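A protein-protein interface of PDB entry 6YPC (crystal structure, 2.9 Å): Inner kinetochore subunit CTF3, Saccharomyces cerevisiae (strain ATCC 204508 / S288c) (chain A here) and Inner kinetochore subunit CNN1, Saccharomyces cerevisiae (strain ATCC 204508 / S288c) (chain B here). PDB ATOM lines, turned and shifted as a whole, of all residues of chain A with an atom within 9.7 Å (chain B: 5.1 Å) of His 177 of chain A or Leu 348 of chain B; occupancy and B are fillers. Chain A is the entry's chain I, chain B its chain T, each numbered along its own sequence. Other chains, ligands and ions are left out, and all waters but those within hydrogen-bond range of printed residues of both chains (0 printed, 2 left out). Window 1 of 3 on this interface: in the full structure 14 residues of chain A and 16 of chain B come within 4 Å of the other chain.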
ATOM      1  N   TRP A 140      18.868  17.164 -38.625  1.00  0.00           N
ATOM      2  CA  TRP A 140      19.573  16.035 -38.044  1.00  0.00           C
ATOM      3  C   TRP A 140      19.605  16.102 -36.521  1.00  0.00           C
ATOM      4  O   TRP A 140      19.561  15.065 -35.855  1.00  0.00           O
ATOM      5  CB  TRP A 140      20.981  15.994 -38.618  1.00  0.00           C
ATOM      6  CG  TRP A 140      21.795  14.929 -38.042  1.00  0.00           C
ATOM      7  CD1 TRP A 140      21.687  13.594 -38.284  1.00  0.00           C
ATOM      8  CD2 TRP A 140      22.858  15.089 -37.107  1.00  0.00           C
ATOM      9  NE1 TRP A 140      22.622  12.906 -37.555  1.00  0.00           N
ATOM     10  CE2 TRP A 140      23.356  13.800 -36.820  1.00  0.00           C
ATOM     11  CE3 TRP A 140      23.444  16.199 -36.485  1.00  0.00           C
ATOM     12  CZ2 TRP A 140      24.419  13.587 -35.939  1.00  0.00           C
ATOM     13  CZ3 TRP A 140      24.505  15.987 -35.607  1.00  0.00           C
ATOM     14  CH2 TRP A 140      24.979  14.689 -35.346  1.00  0.00           C
ATOM     15  N   GLN A 141      19.628  17.311 -35.956  1.00  0.00           N
ATOM     16  CA  GLN A 141      19.740  17.474 -34.510  1.00  0.00           C
ATOM     17  C   GLN A 141      18.507  16.998 -33.741  1.00  0.00           C
ATOM     18  O   GLN A 141      18.605  16.767 -32.534  1.00  0.00           O
ATOM     19  CB  GLN A 141      20.024  18.938 -34.170  1.00  0.00           C
ATOM     20  CG  GLN A 141      21.390  19.414 -34.606  1.00  0.00           C
ATOM     21  CD  GLN A 141      21.533  20.930 -34.513  1.00  0.00           C
ATOM     22  OE1 GLN A 141      22.399  21.439 -33.780  1.00  0.00           O
ATOM     23  NE2 GLN A 141      20.682  21.667 -35.254  1.00  0.00           N
ATOM     24  N   PHE A 142      17.352  16.853 -34.383  1.00  0.00           N
ATOM     25  CA  PHE A 142      16.192  16.314 -33.674  1.00  0.00           C
ATOM     26  C   PHE A 142      16.437  14.857 -33.332  1.00  0.00           C
ATOM     27  O   PHE A 142      16.580  14.018 -34.228  1.00  0.00           O
ATOM     28  CB  PHE A 142      14.932  16.464 -34.510  1.00  0.00           C
ATOM     29  CG  PHE A 142      14.425  17.861 -34.546  1.00  0.00           C
ATOM     30  CD1 PHE A 142      13.848  18.421 -33.425  1.00  0.00           C
ATOM     31  CD2 PHE A 142      14.556  18.637 -35.680  1.00  0.00           C
ATOM     32  CE1 PHE A 142      13.396  19.724 -33.444  1.00  0.00           C
ATOM     33  CE2 PHE A 142      14.097  19.943 -35.695  1.00  0.00           C
ATOM     34  CZ  PHE A 142      13.515  20.482 -34.574  1.00  0.00           C
ATOM     35  N   SER A 143      16.487  14.552 -32.038  1.00  0.00           N
ATOM     36  CA  SER A 143      17.010  13.256 -31.628  1.00  0.00           C
ATOM     37  C   SER A 143      16.260  12.114 -32.303  1.00  0.00           C
ATOM     38  O   SER A 143      16.880  11.127 -32.717  1.00  0.00           O
ATOM     39  CB  SER A 143      16.976  13.122 -30.104  1.00  0.00           C
ATOM     40  OG  SER A 143      15.708  12.727 -29.618  1.00  0.00           O
ATOM     41  N   GLN A 146      17.400  11.370 -36.180  1.00  0.00           N
ATOM     42  CA  GLN A 146      18.798  11.139 -36.510  1.00  0.00           C
ATOM     43  C   GLN A 146      18.993   9.850 -37.295  1.00  0.00           C
ATOM     44  O   GLN A 146      19.735   9.835 -38.278  1.00  0.00           O
ATOM     45  CB  GLN A 146      19.623  11.109 -35.240  1.00  0.00           C
ATOM     46  CG  GLN A 146      20.388  12.360 -35.021  1.00  0.00           C
ATOM     47  CD  GLN A 146      21.412  12.213 -33.914  1.00  0.00           C
ATOM     48  OE1 GLN A 146      21.485  11.173 -33.231  1.00  0.00           O
ATOM     49  NE2 GLN A 146      22.205  13.259 -33.716  1.00  0.00           N
ATOM     50  N   SER A 169      31.207  21.405 -35.767  1.00  0.00           N
ATOM     51  CA  SER A 169      30.893  21.534 -34.356  1.00  0.00           C
ATOM     52  C   SER A 169      29.446  21.152 -34.092  1.00  0.00           C
ATOM     53  O   SER A 169      29.153  20.447 -33.119  1.00  0.00           O
ATOM     54  CB  SER A 169      31.182  22.951 -33.900  1.00  0.00           C
ATOM     55  OG  SER A 169      30.667  23.837 -34.867  1.00  0.00           O
ATOM     56  N   ILE A 170      28.530  21.593 -34.954  1.00  0.00           N
ATOM     57  CA  ILE A 170      27.140  21.153 -34.899  1.00  0.00           C
ATOM     58  C   ILE A 170      27.132  19.647 -34.676  1.00  0.00           C
ATOM     59  O   ILE A 170      26.487  19.140 -33.744  1.00  0.00           O
ATOM     60  CB  ILE A 170      26.387  21.517 -36.191  1.00  0.00           C
ATOM     61  CG1 ILE A 170      26.199  23.023 -36.308  1.00  0.00           C
ATOM     62  CG2 ILE A 170      25.046  20.833 -36.233  1.00  0.00           C
ATOM     63  CD1 ILE A 170      24.878  23.522 -35.788  1.00  0.00           C
ATOM     64  N   ILE A 171      27.881  18.937 -35.521  1.00  0.00           N
ATOM     65  CA  ILE A 171      28.022  17.499 -35.369  1.00  0.00           C
ATOM     66  C   ILE A 171      28.728  17.150 -34.061  1.00  0.00           C
ATOM     67  O   ILE A 171      28.302  16.233 -33.340  1.00  0.00           O
ATOM     68  CB  ILE A 171      28.749  16.911 -36.595  1.00  0.00           C
ATOM     69  CG1 ILE A 171      27.957  17.183 -37.872  1.00  0.00           C
ATOM     70  CG2 ILE A 171      29.002  15.421 -36.438  1.00  0.00           C
ATOM     71  CD1 ILE A 171      28.771  16.994 -39.143  1.00  0.00           C
ATOM     72  N   LYS A 172      29.814  17.858 -33.720  1.00  0.00           N
ATOM     73  CA  LYS A 172      30.571  17.384 -32.569  1.00  0.00           C
ATOM     74  C   LYS A 172      29.821  17.687 -31.277  1.00  0.00           C
ATOM     75  O   LYS A 172      29.747  16.846 -30.376  1.00  0.00           O
ATOM     76  CB  LYS A 172      31.987  17.966 -32.527  1.00  0.00           C
ATOM     77  CG  LYS A 172      32.745  17.443 -31.255  1.00  0.00           C
ATOM     78  CD  LYS A 172      34.162  17.991 -31.013  1.00  0.00           C
ATOM     79  CE  LYS A 172      34.298  19.445 -31.476  1.00  0.00           C
ATOM     80  NZ  LYS A 172      35.520  20.184 -30.969  1.00  0.00           N
ATOM     81  N   ARG A 173      29.238  18.885 -31.179  1.00  0.00           N
ATOM     82  CA  ARG A 173      28.344  19.216 -30.076  1.00  0.00           C
ATOM     83  C   ARG A 173      27.333  18.109 -29.853  1.00  0.00           C
ATOM     84  O   ARG A 173      27.129  17.655 -28.726  1.00  0.00           O
ATOM     85  CB  ARG A 173      27.616  20.537 -30.359  1.00  0.00           C
ATOM     86  CG  ARG A 173      26.265  20.543 -29.697  1.00  0.00           C
ATOM     87  CD  ARG A 173      25.569  21.861 -29.750  1.00  0.00           C
ATOM     88  NE  ARG A 173      24.571  21.871 -28.689  1.00  0.00           N
ATOM     89  CZ  ARG A 173      24.797  22.327 -27.456  1.00  0.00           C
ATOM     90  NH1 ARG A 173      25.975  22.844 -27.151  1.00  0.00           N
ATOM     91  NH2 ARG A 173      23.847  22.280 -26.526  1.00  0.00           N
ATOM     92  N   CYS A 174      26.709  17.645 -30.930  1.00  0.00           N
ATOM     93  CA  CYS A 174      25.597  16.719 -30.792  1.00  0.00           C
ATOM     94  C   CYS A 174      26.066  15.326 -30.405  1.00  0.00           C
ATOM     95  O   CYS A 174      25.380  14.627 -29.654  1.00  0.00           O
ATOM     96  CB  CYS A 174      24.806  16.681 -32.087  1.00  0.00           C
ATOM     97  SG  CYS A 174      23.184  15.994 -31.840  1.00  0.00           S
ATOM     98  N   ALA A 175      27.231  14.904 -30.898  1.00  0.00           N
ATOM     99  CA  ALA A 175      27.753  13.593 -30.518  1.00  0.00           C
ATOM    100  C   ALA A 175      28.022  13.519 -29.020  1.00  0.00           C
ATOM    101  O   ALA A 175      27.540  12.609 -28.338  1.00  0.00           O
ATOM    102  CB  ALA A 175      29.028  13.285 -31.294  1.00  0.00           C
ATOM    103  N   MET A 176      28.793  14.480 -28.494  1.00  0.00           N
ATOM    104  CA  MET A 176      29.181  14.560 -27.090  1.00  0.00           C
ATOM    105  C   MET A 176      28.021  14.892 -26.170  1.00  0.00           C
ATOM    106  O   MET A 176      28.178  14.820 -24.945  1.00  0.00           O
ATOM    107  CB  MET A 176      30.245  15.642 -26.912  1.00  0.00           C
ATOM    108  CG  MET A 176      31.441  15.519 -27.816  1.00  0.00           C
ATOM    109  SD  MET A 176      32.277  13.938 -27.628  1.00  0.00           S
ATOM    110  CE  MET A 176      32.788  13.961 -25.906  1.00  0.00           C
ATOM    111  N   HIS A 177      26.890  15.283 -26.720  1.00  0.00           N
ATOM    112  CA  HIS A 177      25.827  15.899 -25.939  1.00  0.00           C
ATOM    113  C   HIS A 177      25.054  14.843 -25.169  1.00  0.00           C
ATOM    114  O   HIS A 177      24.412  13.989 -25.795  1.00  0.00           O
ATOM    115  CB  HIS A 177      24.908  16.650 -26.883  1.00  0.00           C
ATOM    116  CG  HIS A 177      23.965  17.580 -26.207  1.00  0.00           C
ATOM    117  ND1 HIS A 177      23.398  17.304 -24.985  1.00  0.00           N
ATOM    118  CD2 HIS A 177      23.473  18.779 -26.593  1.00  0.00           C
ATOM    119  CE1 HIS A 177      22.598  18.298 -24.641  1.00  0.00           C
ATOM    120  NE2 HIS A 177      22.629  19.209 -25.598  1.00  0.00           N
ATOM    121  N   PRO A 178      25.067  14.865 -23.836  1.00  0.00           N
ATOM    122  CA  PRO A 178      24.206  13.949 -23.079  1.00  0.00           C
ATOM    123  C   PRO A 178      22.754  14.251 -23.398  1.00  0.00           C
ATOM    124  O   PRO A 178      22.417  15.305 -23.946  1.00  0.00           O
ATOM    125  CB  PRO A 178      24.535  14.269 -21.619  1.00  0.00           C
ATOM    126  CG  PRO A 178      24.922  15.715 -21.646  1.00  0.00           C
ATOM    127  CD  PRO A 178      25.610  15.939 -22.984  1.00  0.00           C
ATOM    128  N   GLY A 179      21.879  13.316 -23.075  1.00  0.00           N
ATOM    129  CA  GLY A 179      20.531  13.467 -23.569  1.00  0.00           C
ATOM    130  C   GLY A 179      20.336  13.098 -25.022  1.00  0.00           C
ATOM    131  O   GLY A 179      19.187  13.077 -25.482  1.00  0.00           O
ATOM    132  N   TYR A 180      21.412  12.830 -25.766  1.00  0.00           N
ATOM    133  CA  TYR A 180      21.358  12.049 -27.000  1.00  0.00           C
ATOM    134  C   TYR A 180      21.947  10.670 -26.735  1.00  0.00           C
ATOM    135  O   TYR A 180      23.009  10.566 -26.118  1.00  0.00           O
ATOM    136  CB  TYR A 180      22.148  12.724 -28.118  1.00  0.00           C
ATOM    137  CG  TYR A 180      21.489  13.940 -28.700  1.00  0.00           C
ATOM    138  CD1 TYR A 180      20.536  13.829 -29.710  1.00  0.00           C
ATOM    139  CD2 TYR A 180      21.833  15.202 -28.262  1.00  0.00           C
ATOM    140  CE1 TYR A 180      19.931  14.959 -30.258  1.00  0.00           C
ATOM    141  CE2 TYR A 180      21.228  16.333 -28.798  1.00  0.00           C
ATOM    142  CZ  TYR A 180      20.281  16.206 -29.788  1.00  0.00           C
ATOM    143  OH  TYR A 180      19.705  17.338 -30.302  1.00  0.00           O
ATOM    144  N   ARG A 181      21.287   9.614 -27.215  1.00  0.00           N
ATOM    145  CA  ARG A 181      21.856   8.273 -27.053  1.00  0.00           C
ATOM    146  C   ARG A 181      22.719   7.838 -28.245  1.00  0.00           C
ATOM    147  O   ARG A 181      23.907   7.539 -28.073  1.00  0.00           O
ATOM    148  CB  ARG A 181      20.750   7.247 -26.781  1.00  0.00           C
ATOM    149  CG  ARG A 181      19.574   7.289 -27.752  1.00  0.00           C
ATOM    150  CD  ARG A 181      18.735   6.006 -27.648  1.00  0.00           C
ATOM    151  NE  ARG A 181      18.009   5.940 -26.378  1.00  0.00           N
ATOM    152  CZ  ARG A 181      17.239   4.922 -26.000  1.00  0.00           C
ATOM    153  NH1 ARG A 181      17.099   3.859 -26.789  1.00  0.00           N
ATOM    154  NH2 ARG A 181      16.618   4.964 -24.824  1.00  0.00           N
ATOM    155  N   ASP A 182      22.149   7.804 -29.459  1.00  0.00           N
ATOM    156  CA  ASP A 182      22.857   7.257 -30.618  1.00  0.00           C
ATOM    157  C   ASP A 182      23.766   8.256 -31.323  1.00  0.00           C
ATOM    158  O   ASP A 182      24.533   7.848 -32.206  1.00  0.00           O
ATOM    159  CB  ASP A 182      21.878   6.714 -31.669  1.00  0.00           C
ATOM    160  CG  ASP A 182      21.007   5.598 -31.148  1.00  0.00           C
ATOM    161  OD1 ASP A 182      21.431   4.914 -30.197  1.00  0.00           O
ATOM    162  OD2 ASP A 182      19.911   5.382 -31.717  1.00  0.00           O
ATOM    163  N   ALA A 183      23.680   9.538 -30.980  1.00  0.00           N
ATOM    164  CA  ALA A 183      24.315  10.566 -31.799  1.00  0.00           C
ATOM    165  C   ALA A 183      25.796  10.325 -32.056  1.00  0.00           C
ATOM    166  O   ALA A 183      26.228  10.556 -33.199  1.00  0.00           O
ATOM    167  CB  ALA A 183      24.092  11.950 -31.174  1.00  0.00           C
ATOM    168  N   PRO A 184      26.617   9.882 -31.088  1.00  0.00           N
ATOM    169  CA  PRO A 184      28.011   9.545 -31.426  1.00  0.00           C
ATOM    170  C   PRO A 184      28.156   8.594 -32.618  1.00  0.00           C
ATOM    171  O   PRO A 184      29.057   8.785 -33.454  1.00  0.00           O
ATOM    172  CB  PRO A 184      28.542   8.921 -30.124  1.00  0.00           C
ATOM    173  CG  PRO A 184      27.353   8.749 -29.242  1.00  0.00           C
ATOM    174  CD  PRO A 184      26.402   9.801 -29.638  1.00  0.00           C
ATOM    175  N   ALA A 187      27.117  10.471 -35.774  1.00  0.00           N
ATOM    176  CA  ALA A 187      28.035  11.587 -35.991  1.00  0.00           C
ATOM    177  C   ALA A 187      29.343  11.113 -36.600  1.00  0.00           C
ATOM    178  O   ALA A 187      29.749  11.612 -37.652  1.00  0.00           O
ATOM    179  CB  ALA A 187      28.303  12.334 -34.682  1.00  0.00           C
ATOM    180  N   THR A 210      37.918  12.230 -30.155  1.00  0.00           N
ATOM    181  CA  THR A 210      37.173  12.730 -28.999  1.00  0.00           C
ATOM    182  C   THR A 210      35.849  12.004 -28.775  1.00  0.00           C
ATOM    183  O   THR A 210      35.346  11.976 -27.647  1.00  0.00           O
ATOM    184  CB  THR A 210      36.908  14.228 -29.175  1.00  0.00           C
ATOM    185  OG1 THR A 210      38.046  14.842 -29.796  1.00  0.00           O
ATOM    186  CG2 THR A 210      36.637  14.888 -27.836  1.00  0.00           C
ATOM    187  N   ILE A 211      35.270  11.433 -29.817  1.00  0.00           N
ATOM    188  CA  ILE A 211      34.087  10.599 -29.715  1.00  0.00           C
ATOM    189  C   ILE A 211      34.557   9.154 -29.834  1.00  0.00           C
ATOM    190  O   ILE A 211      34.794   8.653 -30.941  1.00  0.00           O
ATOM    191  CB  ILE A 211      33.075  10.942 -30.811  1.00  0.00           C
ATOM    192  CG1 ILE A 211      33.185  12.421 -31.138  1.00  0.00           C
ATOM    193  CG2 ILE A 211      31.665  10.533 -30.419  1.00  0.00           C
ATOM    194  CD1 ILE A 211      32.400  12.811 -32.324  1.00  0.00           C
ATOM    195  N   HIS B 280      29.245   8.723 -19.654  1.00  0.00           N
ATOM    196  CA  HIS B 280      28.586   9.346 -20.797  1.00  0.00           C
ATOM    197  C   HIS B 280      27.846  10.625 -20.429  1.00  0.00           C
ATOM    198  O   HIS B 280      27.942  11.621 -21.148  1.00  0.00           O
ATOM    199  CB  HIS B 280      27.611   8.365 -21.452  1.00  0.00           C
ATOM    200  CG  HIS B 280      26.766   8.976 -22.531  1.00  0.00           C
ATOM    201  ND1 HIS B 280      25.394   8.832 -22.575  1.00  0.00           N
ATOM    202  CD2 HIS B 280      27.100   9.722 -23.613  1.00  0.00           C
ATOM    203  CE1 HIS B 280      24.920   9.470 -23.631  1.00  0.00           C
ATOM    204  NE2 HIS B 280      25.934  10.018 -24.279  1.00  0.00           N
ATOM    205  N   LEU B 343      20.758  25.168 -18.589  1.00  0.00           N
ATOM    206  CA  LEU B 343      21.018  23.773 -18.252  1.00  0.00           C
ATOM    207  C   LEU B 343      20.258  22.835 -19.169  1.00  0.00           C
ATOM    208  O   LEU B 343      20.765  21.766 -19.534  1.00  0.00           O
ATOM    209  CB  LEU B 343      20.617  23.478 -16.812  1.00  0.00           C
ATOM    210  CG  LEU B 343      21.699  23.437 -15.758  1.00  0.00           C
ATOM    211  CD1 LEU B 343      22.611  24.637 -15.937  1.00  0.00           C
ATOM    212  CD2 LEU B 343      21.009  23.489 -14.417  1.00  0.00           C
ATOM    213  N   ALA B 344      19.014  23.193 -19.487  1.00  0.00           N
ATOM    214  CA  ALA B 344      18.249  22.422 -20.449  1.00  0.00           C
ATOM    215  C   ALA B 344      19.005  22.318 -21.756  1.00  0.00           C
ATOM    216  O   ALA B 344      19.147  21.230 -22.324  1.00  0.00           O
ATOM    217  CB  ALA B 344      16.885  23.073 -20.668  1.00  0.00           C
ATOM    218  N   HIS B 345      19.540  23.447 -22.216  1.00  0.00           N
ATOM    219  CA  HIS B 345      20.254  23.499 -23.481  1.00  0.00           C
ATOM    220  C   HIS B 345      21.448  22.567 -23.497  1.00  0.00           C
ATOM    221  O   HIS B 345      21.831  22.068 -24.559  1.00  0.00           O
ATOM    222  CB  HIS B 345      20.728  24.919 -23.758  1.00  0.00           C
ATOM    223  CG  HIS B 345      21.537  25.026 -25.007  1.00  0.00           C
ATOM    224  ND1 HIS B 345      22.872  25.370 -25.006  1.00  0.00           N
ATOM    225  CD2 HIS B 345      21.206  24.792 -26.301  1.00  0.00           C
ATOM    226  CE1 HIS B 345      23.325  25.366 -26.248  1.00  0.00           C
ATOM    227  NE2 HIS B 345      22.334  25.019 -27.054  1.00  0.00           N
ATOM    228  N   GLU B 346      22.059  22.326 -22.349  1.00  0.00           N
ATOM    229  CA  GLU B 346      23.265  21.524 -22.345  1.00  0.00           C
ATOM    230  C   GLU B 346      23.040  20.081 -21.944  1.00  0.00           C
ATOM    231  O   GLU B 346      23.964  19.271 -22.081  1.00  0.00           O
ATOM    232  CB  GLU B 346      24.346  22.150 -21.452  1.00  0.00           C
ATOM    233  CG  GLU B 346      25.102  23.197 -22.254  1.00  0.00           C
ATOM    234  CD  GLU B 346      26.001  22.549 -23.339  1.00  0.00           C
ATOM    235  OE1 GLU B 346      25.862  22.974 -24.516  1.00  0.00           O
ATOM    236  OE2 GLU B 346      26.822  21.634 -23.032  1.00  0.00           O
ATOM    237  N   LEU B 347      21.844  19.735 -21.477  1.00  0.00           N
ATOM    238  CA  LEU B 347      21.565  18.377 -21.043  1.00  0.00           C
ATOM    239  C   LEU B 347      20.428  17.722 -21.800  1.00  0.00           C
ATOM    240  O   LEU B 347      20.357  16.494 -21.816  1.00  0.00           O
ATOM    241  CB  LEU B 347      21.233  18.341 -19.543  1.00  0.00           C
ATOM    242  CG  LEU B 347      22.209  18.992 -18.561  1.00  0.00           C
ATOM    243  CD1 LEU B 347      21.825  18.621 -17.150  1.00  0.00           C
ATOM    244  CD2 LEU B 347      23.654  18.594 -18.832  1.00  0.00           C
ATOM    245  N   LEU B 348      19.556  18.478 -22.417  1.00  0.00           N
ATOM    246  CA  LEU B 348      18.446  17.881 -23.141  1.00  0.00           C
ATOM    247  C   LEU B 348      18.690  17.913 -24.643  1.00  0.00           C
ATOM    248  O   LEU B 348      19.365  18.812 -25.151  1.00  0.00           O
ATOM    249  CB  LEU B 348      17.153  18.630 -22.834  1.00  0.00           C
ATOM    250  CG  LEU B 348      16.781  18.417 -21.373  1.00  0.00           C
ATOM    251  CD1 LEU B 348      15.451  19.090 -21.029  1.00  0.00           C
ATOM    252  CD2 LEU B 348      16.745  16.918 -21.119  1.00  0.00           C
ATOM    253  N   PRO B 349      18.143  16.937 -25.371  1.00  0.00           N
ATOM    254  CA  PRO B 349      18.163  17.007 -26.835  1.00  0.00           C
ATOM    255  C   PRO B 349      17.253  18.122 -27.346  1.00  0.00           C
ATOM    256  O   PRO B 349      16.394  18.654 -26.633  1.00  0.00           O
ATOM    257  CB  PRO B 349      17.651  15.631 -27.257  1.00  0.00           C
ATOM    258  CG  PRO B 349      16.781  15.214 -26.096  1.00  0.00           C
ATOM    259  CD  PRO B 349      17.481  15.713 -24.886  1.00  0.00           C
ATOM    260  N   LEU B 350      17.452  18.463 -28.618  1.00  0.00           N
ATOM    261  CA  LEU B 350      16.850  19.660 -29.185  1.00  0.00           C
ATOM    262  C   LEU B 350      15.386  19.813 -28.806  1.00  0.00           C
ATOM    263  O   LEU B 350      14.992  20.802 -28.182  1.00  0.00           O
ATOM    264  CB  LEU B 350      16.994  19.638 -30.709  1.00  0.00           C
ATOM    265  CG  LEU B 350      16.891  21.025 -31.332  1.00  0.00           C
ATOM    266  CD1 LEU B 350      17.992  21.857 -30.727  1.00  0.00           C
ATOM    267  CD2 LEU B 350      17.029  20.958 -32.847  1.00  0.00           C
ATOM    268  N   LEU B 352      13.251  18.452 -26.751  1.00  0.00           N
ATOM    269  CA  LEU B 352      12.880  18.709 -25.372  1.00  0.00           C
ATOM    270  C   LEU B 352      13.240  20.121 -24.961  1.00  0.00           C
ATOM    271  O   LEU B 352      12.591  20.684 -24.079  1.00  0.00           O
ATOM    272  CB  LEU B 352      13.543  17.695 -24.458  1.00  0.00           C
ATOM    273  CG  LEU B 352      12.818  16.367 -24.641  1.00  0.00           C
ATOM    274  CD1 LEU B 352      13.438  15.267 -23.777  1.00  0.00           C
ATOM    275  CD2 LEU B 352      11.328  16.550 -24.338  1.00  0.00           C
ATOM    276  N   GLN B 353      14.261  20.713 -25.579  1.00  0.00           N
ATOM    277  CA  GLN B 353      14.607  22.086 -25.238  1.00  0.00           C
ATOM    278  C   GLN B 353      13.463  23.017 -25.578  1.00  0.00           C
ATOM    279  O   GLN B 353      13.030  23.816 -24.738  1.00  0.00           O
ATOM    280  CB  GLN B 353      15.883  22.518 -25.948  1.00  0.00           C
ATOM    281  CG  GLN B 353      17.078  21.744 -25.493  1.00  0.00           C
ATOM    282  CD  GLN B 353      18.323  22.112 -26.248  1.00  0.00           C
ATOM    283  OE1 GLN B 353      18.366  23.128 -26.937  1.00  0.00           O
ATOM    284  NE2 GLN B 353      19.357  21.288 -26.118  1.00  0.00           N
ATOM    285  N   ILE B 356      10.646  22.363 -22.695  1.00  0.00           N
ATOM    286  CA  ILE B 356      11.015  23.008 -21.439  1.00  0.00           C
ATOM    287  C   ILE B 356      10.958  24.523 -21.537  1.00  0.00           C
ATOM    288  O   ILE B 356      10.572  25.199 -20.579  1.00  0.00           O
ATOM    289  CB  ILE B 356      12.414  22.534 -21.017  1.00  0.00           C
ATOM    290  CG1 ILE B 356      12.354  21.090 -20.564  1.00  0.00           C
ATOM    291  CG2 ILE B 356      12.941  23.366 -19.880  1.00  0.00           C
ATOM    292  CD1 ILE B 356      11.927  20.932 -19.131  1.00  0.00           C
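Hydrophobic or aromatic side chains of chain B that line the printed part of chain A: His 280, His 345, Pro 349 and Leu 350. Among the printed residues, 17 pairs touch across the chains.
His 177 of chain A touches just these residues of chain B: His 345 (3.1 Å), Glu 346 (3.1 Å), Leu 347 (3.6 Å), Leu 348 (3.3 Å) and Gln 353 (3.9 Å). Of chain A, only His 177 (3.3 Å) comes within 4 Å of Leu 348 of chain B. Ala 344 of chain B touches none of the printed residues of chain A. Of the printed residues of chain A, Pro 349 of chain B touches Ser 143 (3.9 Å), Gly 179 (3.2 Å) and Tyr 180 (3.7 Å). Of the printed residues of chain B, Pro 178 of chain A touches Glu 346 (3.7 Å) and Leu 347 (3.2 Å). Of the printed residues of chain A, His 345 of chain B touches Arg 173 (2.8 Å) and His 177 (3.1 Å). Of the printed residues of chain B, Gln 141 of chain A touches Leu 350. Lys 172 of chain A touches none of the printed residues of chain B. Ile 211 of chain A touches none of the printed residues of chain B.
NE2 of Gln 353 of chain B lies within hydrogen-bond range of O of His 345 of chain B, at 3.0 Å. The backbone carbonyl oxygen (O) of Leu 348 of chain B is in hydrogen-bond range of the side-chain amide nitrogen (NE2) of Gln 353 of chain B (2.7 Å). OH of Tyr 180 of chain A is in hydrogen-bond range of O of Gln 141 of chain A, at 2.6 Å. The guanidinium group (NH2) of Arg 173 of chain A lies within hydrogen-bond range of a ring nitrogen (NE2) of His 177 of chain A (3.4 Å).
The backbone carbonyl oxygen (O) of Tyr 180 of chain A sits close to a ring nitrogen (NE2) of His 280 of chain B, 3.5 Å away. NH2 of Arg 173 of chain A is in hydrogen-bond range of O of His 345 of chain B (2.8 Å). NE2 of His 177 of chain A is in hydrogen-bond range of O of His 345 of chain B. The side-chain carboxylate (OE1) of Glu 346 of chain B lies within salt-bridge range of the guanidinium group (NH1) of Arg 173 of chain A. NE2 of His 177 of chain A sits close to O of Leu 348 of chain B (3.3 Å). The backbone NH (N) of Leu 350 of chain B sits at hydrogen-bond distance from the side-chain hydroxyl (OH) of Tyr 180 of chain A, at 3.0 Å. The backbone carbonyl oxygen (O) of Leu 347 of chain B lies close to the backbone carbonyl oxygen (O) of Pro 178 of chain A (3.2 Å).
Among the printed residues, merely in contact across the chains: His 177 of chain A with Glu 346 of chain B (3.1 Å), Gly 179 of chain A with Pro 349 of chain B (3.2 Å), Gly 179 of chain A with Leu 347 of chain B (3.5 Å), His 177 of chain A with Leu 347 of chain B (3.6 Å), Tyr 180 of chain A with Pro 349 of chain B (3.7 Å), Pro 178 of chain A with Glu 346 of chain B (3.7 Å), Gln 141 of chain A with Leu 350 of chain B (3.8 Å), Ser 143 of chain A with Pro 349 of chain B (3.9 Å), Phe 142 of chain A with Leu 350 of chain B (3.9 Å) and His 177 of chain A with Gln 353 of chain B (3.9 Å).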
